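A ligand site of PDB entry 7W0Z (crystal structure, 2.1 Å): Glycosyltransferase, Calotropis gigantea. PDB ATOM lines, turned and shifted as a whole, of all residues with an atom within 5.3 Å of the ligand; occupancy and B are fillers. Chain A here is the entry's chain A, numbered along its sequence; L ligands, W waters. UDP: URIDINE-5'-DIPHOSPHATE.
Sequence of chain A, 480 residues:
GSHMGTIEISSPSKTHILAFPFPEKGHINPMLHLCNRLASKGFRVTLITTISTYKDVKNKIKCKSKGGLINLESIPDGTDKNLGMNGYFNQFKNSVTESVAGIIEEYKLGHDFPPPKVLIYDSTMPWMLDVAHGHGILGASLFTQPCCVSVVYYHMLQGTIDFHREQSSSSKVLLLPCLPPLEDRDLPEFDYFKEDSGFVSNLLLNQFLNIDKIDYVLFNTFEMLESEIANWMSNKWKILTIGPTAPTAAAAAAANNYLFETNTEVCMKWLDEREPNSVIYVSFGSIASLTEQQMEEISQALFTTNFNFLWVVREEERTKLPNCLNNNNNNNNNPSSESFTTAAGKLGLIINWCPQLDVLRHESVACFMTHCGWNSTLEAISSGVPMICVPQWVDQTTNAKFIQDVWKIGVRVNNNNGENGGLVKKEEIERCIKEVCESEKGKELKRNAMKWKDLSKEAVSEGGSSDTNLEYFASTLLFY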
ATOM      1  N   GLU A  24       7.044   7.638 -35.039  1.00  0.00           N
ATOM      2  CA  GLU A  24       7.006   6.318 -34.447  1.00  0.00           C
ATOM      3  C   GLU A  24       5.617   6.191 -33.828  1.00  0.00           C
ATOM      4  O   GLU A  24       5.080   7.189 -33.335  1.00  0.00           O
ATOM      5  CB  GLU A  24       8.136   6.144 -33.414  1.00  0.00           C
ATOM      6  CG  GLU A  24       8.347   4.766 -32.790  1.00  0.00           C
ATOM      7  CD  GLU A  24       7.517   4.506 -31.520  1.00  0.00           C
ATOM      8  OE1 GLU A  24       7.005   5.461 -30.871  1.00  0.00           O
ATOM      9  OE2 GLU A  24       7.434   3.328 -31.143  1.00  0.00           O
ATOM     10  N   LYS A  25       5.027   4.990 -33.890  1.00  0.00           N
ATOM     11  CA  LYS A  25       3.601   4.862 -33.602  1.00  0.00           C
ATOM     12  C   LYS A  25       3.266   5.217 -32.156  1.00  0.00           C
ATOM     13  O   LYS A  25       2.174   5.728 -31.898  1.00  0.00           O
ATOM     14  CB  LYS A  25       3.120   3.455 -33.912  1.00  0.00           C
ATOM     15  CG  LYS A  25       3.287   3.068 -35.359  1.00  0.00           C
ATOM     16  CD  LYS A  25       2.173   2.153 -35.780  1.00  0.00           C
ATOM     17  CE  LYS A  25       2.065   2.141 -37.278  1.00  0.00           C
ATOM     18  NZ  LYS A  25       3.190   1.366 -37.812  1.00  0.00           N
ATOM     19  N   GLY A  26       4.155   4.914 -31.211  1.00  0.00           N
ATOM     20  CA  GLY A  26       3.911   5.278 -29.823  1.00  0.00           C
ATOM     21  C   GLY A  26       4.028   6.763 -29.541  1.00  0.00           C
ATOM     22  O   GLY A  26       3.660   7.206 -28.441  1.00  0.00           O
ATOM     23  N   ASN A  29       0.522   8.053 -32.257  1.00  0.00           N
ATOM     24  CA  ASN A  29      -0.858   7.734 -31.865  1.00  0.00           C
ATOM     25  C   ASN A  29      -1.395   8.645 -30.767  1.00  0.00           C
ATOM     26  O   ASN A  29      -2.555   9.078 -30.883  1.00  0.00           O
ATOM     27  CB  ASN A  29      -0.962   6.272 -31.414  1.00  0.00           C
ATOM     28  CG  ASN A  29      -0.998   5.313 -32.555  1.00  0.00           C
ATOM     29  OD1 ASN A  29      -0.959   5.712 -33.722  1.00  0.00           O
ATOM     30  ND2 ASN A  29      -1.042   4.014 -32.231  1.00  0.00           N
ATOM     31  N   GLU A 261      -7.240   1.151 -37.417  1.00  0.00           N
ATOM     32  CA  GLU A 261      -6.059   0.326 -37.611  1.00  0.00           C
ATOM     33  C   GLU A 261      -6.336  -0.754 -38.647  1.00  0.00           C
ATOM     34  O   GLU A 261      -7.483  -1.066 -38.948  1.00  0.00           O
ATOM     35  CB  GLU A 261      -5.607  -0.313 -36.291  1.00  0.00           C
ATOM     36  CG  GLU A 261      -5.056   0.659 -35.261  1.00  0.00           C
ATOM     37  CD  GLU A 261      -3.662   1.145 -35.604  1.00  0.00           C
ATOM     38  OE1 GLU A 261      -3.168   0.767 -36.695  1.00  0.00           O
ATOM     39  OE2 GLU A 261      -3.048   1.876 -34.787  1.00  0.00           O
ATOM     40  N   TYR A 281      -4.141 -11.598 -24.936  1.00  0.00           N
ATOM     41  CA  TYR A 281      -3.703 -10.699 -25.997  1.00  0.00           C
ATOM     42  C   TYR A 281      -2.209 -10.448 -25.807  1.00  0.00           C
ATOM     43  O   TYR A 281      -1.772 -10.046 -24.723  1.00  0.00           O
ATOM     44  CB  TYR A 281      -4.492  -9.383 -25.948  1.00  0.00           C
ATOM     45  CG  TYR A 281      -3.945  -8.338 -26.885  1.00  0.00           C
ATOM     46  CD1 TYR A 281      -3.715  -8.644 -28.215  1.00  0.00           C
ATOM     47  CD2 TYR A 281      -3.646  -7.064 -26.441  1.00  0.00           C
ATOM     48  CE1 TYR A 281      -3.202  -7.705 -29.088  1.00  0.00           C
ATOM     49  CE2 TYR A 281      -3.133  -6.103 -27.303  1.00  0.00           C
ATOM     50  CZ  TYR A 281      -2.914  -6.430 -28.634  1.00  0.00           C
ATOM     51  OH  TYR A 281      -2.408  -5.501 -29.515  1.00  0.00           O
ATOM     52  N   SER A 283       1.247  -8.598 -27.432  1.00  0.00           N
ATOM     53  CA  SER A 283       1.849  -7.667 -28.366  1.00  0.00           C
ATOM     54  C   SER A 283       3.066  -7.031 -27.723  1.00  0.00           C
ATOM     55  O   SER A 283       3.041  -6.675 -26.546  1.00  0.00           O
ATOM     56  CB  SER A 283       0.856  -6.580 -28.794  1.00  0.00           C
ATOM     57  OG  SER A 283       1.503  -5.558 -29.538  1.00  0.00           O
ATOM     58  N   PHE A 284       4.134  -6.876 -28.508  1.00  0.00           N
ATOM     59  CA  PHE A 284       5.343  -6.194 -28.055  1.00  0.00           C
ATOM     60  C   PHE A 284       5.518  -4.856 -28.760  1.00  0.00           C
ATOM     61  O   PHE A 284       6.638  -4.342 -28.867  1.00  0.00           O
ATOM     62  CB  PHE A 284       6.552  -7.121 -28.222  1.00  0.00           C
ATOM     63  CG  PHE A 284       6.553  -8.268 -27.233  1.00  0.00           C
ATOM     64  CD1 PHE A 284       5.741  -9.386 -27.440  1.00  0.00           C
ATOM     65  CD2 PHE A 284       7.325  -8.221 -26.086  1.00  0.00           C
ATOM     66  CE1 PHE A 284       5.711 -10.415 -26.510  1.00  0.00           C
ATOM     67  CE2 PHE A 284       7.307  -9.275 -25.164  1.00  0.00           C
ATOM     68  CZ  PHE A 284       6.496 -10.356 -25.380  1.00  0.00           C
ATOM     69  N   GLY A 285       4.418  -4.275 -29.227  1.00  0.00           N
ATOM     70  CA  GLY A 285       4.457  -2.918 -29.747  1.00  0.00           C
ATOM     71  C   GLY A 285       4.986  -2.837 -31.157  1.00  0.00           C
ATOM     72  O   GLY A 285       4.960  -3.803 -31.933  1.00  0.00           O
ATOM     73  N   SER A 286       5.471  -1.641 -31.506  1.00  0.00           N
ATOM     74  CA  SER A 286       5.740  -1.291 -32.894  1.00  0.00           C
ATOM     75  C   SER A 286       7.204  -1.434 -33.291  1.00  0.00           C
ATOM     76  O   SER A 286       7.493  -1.430 -34.493  1.00  0.00           O
ATOM     77  CB  SER A 286       5.267   0.141 -33.177  1.00  0.00           C
ATOM     78  OG  SER A 286       6.102   1.077 -32.505  1.00  0.00           O
ATOM     79  N   ILE A 287       8.130  -1.541 -32.343  1.00  0.00           N
ATOM     80  CA  ILE A 287       9.546  -1.539 -32.725  1.00  0.00           C
ATOM     81  C   ILE A 287      10.363  -2.615 -32.022  1.00  0.00           C
ATOM     82  O   ILE A 287      11.382  -3.053 -32.566  1.00  0.00           O
ATOM     83  CB  ILE A 287      10.168  -0.154 -32.505  1.00  0.00           C
ATOM     84  CG1 ILE A 287      10.015   0.304 -31.072  1.00  0.00           C
ATOM     85  CG2 ILE A 287       9.530   0.906 -33.410  1.00  0.00           C
ATOM     86  CD1 ILE A 287      10.511   1.738 -30.879  1.00  0.00           C
ATOM     87  N   ALA A 288       9.966  -3.052 -30.817  1.00  0.00           N
ATOM     88  CA  ALA A 288      10.748  -4.092 -30.128  1.00  0.00           C
ATOM     89  C   ALA A 288      10.837  -5.368 -30.964  1.00  0.00           C
ATOM     90  O   ALA A 288       9.872  -5.761 -31.628  1.00  0.00           O
ATOM     91  CB  ALA A 288      10.134  -4.419 -28.769  1.00  0.00           C
ATOM     92  N   VAL A 312       0.199 -10.584 -31.767  1.00  0.00           N
ATOM     93  CA  VAL A 312       0.646  -9.702 -32.840  1.00  0.00           C
ATOM     94  C   VAL A 312       2.114  -9.995 -33.094  1.00  0.00           C
ATOM     95  O   VAL A 312       2.957  -9.781 -32.225  1.00  0.00           O
ATOM     96  CB  VAL A 312       0.446  -8.233 -32.468  1.00  0.00           C
ATOM     97  CG1 VAL A 312       1.154  -7.343 -33.487  1.00  0.00           C
ATOM     98  CG2 VAL A 312      -1.073  -7.907 -32.358  1.00  0.00           C
ATOM     99  N   TRP A 353      -0.817  -7.130 -37.142  1.00  0.00           N
ATOM    100  CA  TRP A 353      -1.233  -5.870 -36.530  1.00  0.00           C
ATOM    101  C   TRP A 353      -2.721  -6.002 -36.205  1.00  0.00           C
ATOM    102  O   TRP A 353      -3.432  -6.778 -36.828  1.00  0.00           O
ATOM    103  CB  TRP A 353      -1.023  -4.665 -37.444  1.00  0.00           C
ATOM    104  CG  TRP A 353      -0.850  -3.349 -36.733  1.00  0.00           C
ATOM    105  CD1 TRP A 353      -1.695  -2.274 -36.757  1.00  0.00           C
ATOM    106  CD2 TRP A 353       0.241  -2.985 -35.892  1.00  0.00           C
ATOM    107  NE1 TRP A 353      -1.186  -1.255 -35.982  1.00  0.00           N
ATOM    108  CE2 TRP A 353       0.002  -1.670 -35.441  1.00  0.00           C
ATOM    109  CE3 TRP A 353       1.405  -3.646 -35.462  1.00  0.00           C
ATOM    110  CZ2 TRP A 353       0.888  -0.995 -34.590  1.00  0.00           C
ATOM    111  CZ3 TRP A 353       2.275  -2.986 -34.617  1.00  0.00           C
ATOM    112  CH2 TRP A 353       2.016  -1.664 -34.197  1.00  0.00           C
ATOM    113  N   CYS A 354      -3.184  -5.210 -35.235  1.00  0.00           N
ATOM    114  CA  CYS A 354      -4.569  -5.289 -34.793  1.00  0.00           C
ATOM    115  C   CYS A 354      -4.999  -3.920 -34.314  1.00  0.00           C
ATOM    116  O   CYS A 354      -4.153  -3.052 -34.078  1.00  0.00           O
ATOM    117  CB  CYS A 354      -4.730  -6.326 -33.662  1.00  0.00           C
ATOM    118  SG  CYS A 354      -4.162  -5.749 -32.026  1.00  0.00           S
ATOM    119  N   PRO A 355      -6.322  -3.677 -34.157  1.00  0.00           N
ATOM    120  CA  PRO A 355      -6.757  -2.422 -33.534  1.00  0.00           C
ATOM    121  C   PRO A 355      -6.683  -2.549 -32.022  1.00  0.00           C
ATOM    122  O   PRO A 355      -7.644  -2.962 -31.375  1.00  0.00           O
ATOM    123  CB  PRO A 355      -8.198  -2.264 -34.035  1.00  0.00           C
ATOM    124  CG  PRO A 355      -8.667  -3.669 -34.251  1.00  0.00           C
ATOM    125  CD  PRO A 355      -7.467  -4.494 -34.627  1.00  0.00           C
ATOM    126  N   GLN A 356      -5.529  -2.165 -31.459  1.00  0.00           N
ATOM    127  CA  GLN A 356      -5.231  -2.569 -30.089  1.00  0.00           C
ATOM    128  C   GLN A 356      -6.271  -2.063 -29.099  1.00  0.00           C
ATOM    129  O   GLN A 356      -6.671  -2.787 -28.187  1.00  0.00           O
ATOM    130  CB  GLN A 356      -3.837  -2.092 -29.673  1.00  0.00           C
ATOM    131  CG  GLN A 356      -3.593  -2.269 -28.161  1.00  0.00           C
ATOM    132  CD  GLN A 356      -2.110  -2.232 -27.785  1.00  0.00           C
ATOM    133  OE1 GLN A 356      -1.662  -1.326 -27.073  1.00  0.00           O
ATOM    134  NE2 GLN A 356      -1.373  -3.209 -28.264  1.00  0.00           N
ATOM    135  N   LEU A 357      -6.721  -0.818 -29.250  1.00  0.00           N
ATOM    136  CA  LEU A 357      -7.692  -0.280 -28.301  1.00  0.00           C
ATOM    137  C   LEU A 357      -9.017  -1.027 -28.368  1.00  0.00           C
ATOM    138  O   LEU A 357      -9.645  -1.311 -27.337  1.00  0.00           O
ATOM    139  CB  LEU A 357      -7.888   1.225 -28.552  1.00  0.00           C
ATOM    140  CG  LEU A 357      -8.568   2.041 -27.449  1.00  0.00           C
ATOM    141  CD1 LEU A 357      -7.975   1.750 -26.088  1.00  0.00           C
ATOM    142  CD2 LEU A 357      -8.487   3.535 -27.771  1.00  0.00           C
ATOM    143  N   HIS A 371       4.906  -5.507 -23.740  1.00  0.00           N
ATOM    144  CA  HIS A 371       6.250  -5.002 -23.476  1.00  0.00           C
ATOM    145  C   HIS A 371       6.247  -3.794 -22.563  1.00  0.00           C
ATOM    146  O   HIS A 371       7.324  -3.263 -22.258  1.00  0.00           O
ATOM    147  CB  HIS A 371       6.958  -4.668 -24.799  1.00  0.00           C
ATOM    148  CG  HIS A 371       6.460  -3.426 -25.456  1.00  0.00           C
ATOM    149  ND1 HIS A 371       5.127  -3.181 -25.673  1.00  0.00           N
ATOM    150  CD2 HIS A 371       7.125  -2.357 -25.968  1.00  0.00           C
ATOM    151  CE1 HIS A 371       4.983  -2.012 -26.283  1.00  0.00           C
ATOM    152  NE2 HIS A 371       6.183  -1.496 -26.470  1.00  0.00           N
ATOM    153  N   GLY A 373       5.321  -0.691 -23.144  1.00  0.00           N
ATOM    154  CA  GLY A 373       5.394   0.664 -23.679  1.00  0.00           C
ATOM    155  C   GLY A 373       4.318   1.509 -23.013  1.00  0.00           C
ATOM    156  O   GLY A 373       3.337   0.948 -22.541  1.00  0.00           O
ATOM    157  N   TRP A 374       4.476   2.834 -22.925  1.00  0.00           N
ATOM    158  CA  TRP A 374       3.527   3.582 -22.100  1.00  0.00           C
ATOM    159  C   TRP A 374       2.127   3.641 -22.724  1.00  0.00           C
ATOM    160  O   TRP A 374       1.133   3.563 -22.002  1.00  0.00           O
ATOM    161  CB  TRP A 374       4.037   4.994 -21.811  1.00  0.00           C
ATOM    162  CG  TRP A 374       3.017   5.810 -21.038  1.00  0.00           C
ATOM    163  CD1 TRP A 374       2.399   6.960 -21.445  1.00  0.00           C
ATOM    164  CD2 TRP A 374       2.511   5.528 -19.719  1.00  0.00           C
ATOM    165  NE1 TRP A 374       1.530   7.389 -20.473  1.00  0.00           N
ATOM    166  CE2 TRP A 374       1.579   6.536 -19.408  1.00  0.00           C
ATOM    167  CE3 TRP A 374       2.744   4.512 -18.772  1.00  0.00           C
ATOM    168  CZ2 TRP A 374       0.888   6.566 -18.181  1.00  0.00           C
ATOM    169  CZ3 TRP A 374       2.062   4.539 -17.577  1.00  0.00           C
ATOM    170  CH2 TRP A 374       1.130   5.561 -17.285  1.00  0.00           C
ATOM    171  N   ASN A 375       2.019   3.770 -24.057  1.00  0.00           N
ATOM    172  CA  ASN A 375       0.691   3.789 -24.668  1.00  0.00           C
ATOM    173  C   ASN A 375      -0.060   2.481 -24.421  1.00  0.00           C
ATOM    174  O   ASN A 375      -1.242   2.491 -24.074  1.00  0.00           O
ATOM    175  CB  ASN A 375       0.768   4.038 -26.174  1.00  0.00           C
ATOM    176  CG  ASN A 375       1.274   5.419 -26.518  1.00  0.00           C
ATOM    177  OD1 ASN A 375       0.557   6.419 -26.372  1.00  0.00           O
ATOM    178  ND2 ASN A 375       2.507   5.480 -26.954  1.00  0.00           N
ATOM    179  N   SER A 376       0.626   1.345 -24.613  1.00  0.00           N
ATOM    180  CA  SER A 376       0.030   0.050 -24.299  1.00  0.00           C
ATOM    181  C   SER A 376      -0.400  -0.027 -22.837  1.00  0.00           C
ATOM    182  O   SER A 376      -1.502  -0.503 -22.528  1.00  0.00           O
ATOM    183  CB  SER A 376       1.024  -1.068 -24.630  1.00  0.00           C
ATOM    184  OG  SER A 376       1.153  -1.184 -26.050  1.00  0.00           O
ATOM    185  N   THR A 377       0.467   0.417 -21.919  1.00  0.00           N
ATOM    186  CA  THR A 377       0.140   0.416 -20.493  1.00  0.00           C
ATOM    187  C   THR A 377      -1.100   1.264 -20.206  1.00  0.00           C
ATOM    188  O   THR A 377      -2.053   0.799 -19.562  1.00  0.00           O
ATOM    189  CB  THR A 377       1.326   0.929 -19.671  1.00  0.00           C
ATOM    190  OG1 THR A 377       2.461   0.081 -19.873  1.00  0.00           O
ATOM    191  CG2 THR A 377       1.016   0.930 -18.197  1.00  0.00           C
ATOM    192  N   GLU A 379      -3.372   2.436 -22.318  1.00  0.00           N
ATOM    193  CA  GLU A 379      -4.545   1.877 -22.996  1.00  0.00           C
ATOM    194  C   GLU A 379      -5.132   0.705 -22.204  1.00  0.00           C
ATOM    195  O   GLU A 379      -6.354   0.618 -22.041  1.00  0.00           O
ATOM    196  CB  GLU A 379      -4.196   1.464 -24.419  1.00  0.00           C
ATOM    197  CG  GLU A 379      -4.061   2.648 -25.369  1.00  0.00           C
ATOM    198  CD  GLU A 379      -3.302   2.312 -26.644  1.00  0.00           C
ATOM    199  OE1 GLU A 379      -3.213   1.118 -26.993  1.00  0.00           O
ATOM    200  OE2 GLU A 379      -2.775   3.242 -27.300  1.00  0.00           O
ATOM    201  N   TRP A 393      13.096  -2.364 -23.058  1.00  0.00           N
ATOM    202  CA  TRP A 393      14.122  -1.331 -22.846  1.00  0.00           C
ATOM    203  C   TRP A 393      13.482   0.024 -22.583  1.00  0.00           C
ATOM    204  O   TRP A 393      12.258   0.167 -22.549  1.00  0.00           O
ATOM    205  CB  TRP A 393      15.086  -1.259 -24.034  1.00  0.00           C
ATOM    206  CG  TRP A 393      14.476  -1.657 -25.326  1.00  0.00           C
ATOM    207  CD1 TRP A 393      14.662  -2.824 -26.019  1.00  0.00           C
ATOM    208  CD2 TRP A 393      13.575  -0.876 -26.111  1.00  0.00           C
ATOM    209  NE1 TRP A 393      13.926  -2.815 -27.179  1.00  0.00           N
ATOM    210  CE2 TRP A 393      13.249  -1.623 -27.261  1.00  0.00           C
ATOM    211  CE3 TRP A 393      13.007   0.391 -25.948  1.00  0.00           C
ATOM    212  CZ2 TRP A 393      12.395  -1.150 -28.237  1.00  0.00           C
ATOM    213  CZ3 TRP A 393      12.145   0.858 -26.923  1.00  0.00           C
ATOM    214  CH2 TRP A 393      11.845   0.093 -28.046  1.00  0.00           C
ATOM    215  N   GLN A 396      10.174   0.903 -20.416  1.00  0.00           N
ATOM    216  CA  GLN A 396       9.325  -0.261 -20.186  1.00  0.00           C
ATOM    217  C   GLN A 396       9.651  -0.943 -18.864  1.00  0.00           C
ATOM    218  O   GLN A 396       8.740  -1.498 -18.209  1.00  0.00           O
ATOM    219  CB  GLN A 396       9.467  -1.250 -21.347  1.00  0.00           C
ATOM    220  CG  GLN A 396       9.031  -0.645 -22.692  1.00  0.00           C
ATOM    221  CD  GLN A 396       9.747  -1.269 -23.896  1.00  0.00           C
ATOM    222  OE1 GLN A 396      10.328  -2.356 -23.809  1.00  0.00           O
ATOM    223  NE2 GLN A 396       9.669  -0.584 -25.035  1.00  0.00           N
HETATM  224  N1  UDP L   1      -0.620  -0.875 -31.555  1.00  0.00           N
HETATM  225  C2  UDP L   1      -1.605  -1.169 -32.359  1.00  0.00           C
HETATM  226  N3  UDP L   1      -1.767  -2.371 -32.853  1.00  0.00           N
HETATM  227  C4  UDP L   1      -0.908  -3.314 -32.530  1.00  0.00           C
HETATM  228  C5  UDP L   1       0.169  -3.067 -31.683  1.00  0.00           C
HETATM  229  C6  UDP L   1       0.296  -1.766 -31.192  1.00  0.00           C
HETATM  230  O2  UDP L   1      -2.536  -0.186 -32.695  1.00  0.00           O
HETATM  231  O4  UDP L   1      -1.120  -4.565 -33.087  1.00  0.00           O
HETATM  232  C1' UDP L   1      -0.545   0.529 -31.085  1.00  0.00           C
HETATM  233  C2' UDP L   1      -0.887   0.648 -29.590  1.00  0.00           C
HETATM  234  O2' UDP L   1      -2.231   0.883 -29.444  1.00  0.00           O
HETATM  235  C3' UDP L   1      -0.007   1.847 -29.150  1.00  0.00           C
HETATM  236  C4' UDP L   1       1.062   1.805 -29.918  1.00  0.00           C
HETATM  237  O4' UDP L   1       0.685   0.980 -31.254  1.00  0.00           O
HETATM  238  O3' UDP L   1      -0.777   3.112 -29.417  1.00  0.00           O
HETATM  239  C5' UDP L   1       2.240   1.120 -29.252  1.00  0.00           C
HETATM  240  O5' UDP L   1       2.956   2.122 -28.568  1.00  0.00           O
HETATM  241  PA  UDP L   1       3.667   1.743 -27.148  1.00  0.00           P
HETATM  242  O1A UDP L   1       3.919   2.993 -26.328  1.00  0.00           O
HETATM  243  O2A UDP L   1       2.849   0.769 -26.346  1.00  0.00           O
HETATM  244  O3A UDP L   1       5.055   0.949 -27.485  1.00  0.00           O
HETATM  245  PB  UDP L   1       6.112   1.247 -28.723  1.00  0.00           P
HETATM  246  O1B UDP L   1       6.299   2.747 -28.856  1.00  0.00           O
HETATM  247  O2B UDP L   1       5.617   0.616 -30.003  1.00  0.00           O
HETATM  248  O3B UDP L   1       7.360   0.534 -28.249  1.00  0.00           O
HETATM  249  O   HOH W   1       7.941  -1.763 -29.423  1.00  0.00           O
HETATM  250  O   HOH W   2       1.319  -3.087 -28.307  1.00  0.00           O
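OE2 of Glu 261 sits close to O2 of the ligand (3.0 Å). A nitrogen (N3) of the ligand sits close to the indole nitrogen of Trp 353. Merely in contact with the ligand: Gly 26 (3.5 Å), Tyr 281 (3.9 Å), Ser 283 (3.5 Å), Gly 285 (3.7 Å), Ile 287 (3.9 Å), Val 312 (3.4 Å) and Gly 373 (3.7 Å). Hydrophobic or aromatic side chains within 4 Å of the ligand: Ile 287, Val 312, Trp 353 and His 371.
OE1 of Glu 261 lies within hydrogen-bond range of NE1 of Trp 353. The side-chain hydroxyl (OG1) of Thr 377 lies within hydrogen-bond range of the backbone carbonyl oxygen (O) of Gly 373 (2.9 Å). The side-chain hydroxyl (OG) of Ser 283 lies within hydrogen-bond range of the backbone NH (N) of Gly 285, at 3.2 Å. OH of Tyr 281 sits at hydrogen-bond distance from NE2 of Gln 356, 2.8 Å away. The side-chain hydroxyl (OG) of Ser 286 is in hydrogen-bond range of the side-chain carboxylate (OE2) of Glu 24 (2.9 Å). The backbone carbonyl oxygen (O) of Gly 26 sits at hydrogen-bond distance from the side-chain amide nitrogen (ND2) of Asn 375. The side-chain amide oxygen (OE1) of Gln 356 is in hydrogen-bond range of the side-chain hydroxyl (OG) of Ser 376 (3.0 Å). OE1 of Glu 24 lies within hydrogen-bond range of N of Gly 26 (2.9 Å).
Water W2 lies within hydrogen-bond range of the side-chain amide nitrogen (NE2) of Gln 356 (2.7 Å), the side-chain hydroxyl (OG) of Ser 283 (2.8 Å), the side-chain hydroxyl (OG) of Ser 376 (3.0 Å) and the backbone NH (N) of Gly 285 (3.4 Å).
An oxygen (O2A) of the ligand lies within hydrogen-bond range of the side-chain hydroxyl of Ser 376 (2.6 Å). The backbone NH (N) of Cys 354 sits at hydrogen-bond distance from an oxygen (O4) of the ligand (3.0 Å). O1B of the ligand lies close to OE2 of Glu 24. A nitrogen (N3) of the ligand lies within hydrogen-bond range of the backbone carbonyl oxygen (O) of Cys 354, at 2.8 Å. The backbone NH of Ser 286 sits at hydrogen-bond distance from an oxygen (O2B) of the ligand, 2.7 Å away. The side-chain carboxylate of Glu 379 is in hydrogen-bond range of an oxygen (O2') of the ligand (2.7 Å). O2A of the ligand lies within hydrogen-bond range of N of Ser 376 (2.9 Å). The side-chain amide nitrogen (ND2) of Asn 29 sits at hydrogen-bond distance from an oxygen (O3') of the ligand (3.0 Å). The side-chain amide oxygen (OE1) of Gln 356 sits at hydrogen-bond distance from an oxygen (O2') of the ligand (3.3 Å). The side-chain sulfur (SG) of Cys 354 lies within hydrogen-bond range of an oxygen (O4) of the ligand (3.4 Å). The side-chain amide nitrogen (ND2) of Asn 375 lies within hydrogen-bond range of an oxygen (O1A) of the ligand (2.9 Å). An oxygen (O2B) of the ligand is in hydrogen-bond range of the side-chain hydroxyl of Ser 286, 2.6 Å away. The backbone NH (N) of Trp 374 lies within hydrogen-bond range of an oxygen (O1A) of the ligand, at 3.5 Å. The backbone NH of Asn 375 lies within hydrogen-bond range of an oxygen (O1A) of the ligand, at 3.1 Å. An oxygen (O3A) of the ligand lies within hydrogen-bond range of a ring nitrogen (NE2) of His 371 (2.9 Å).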
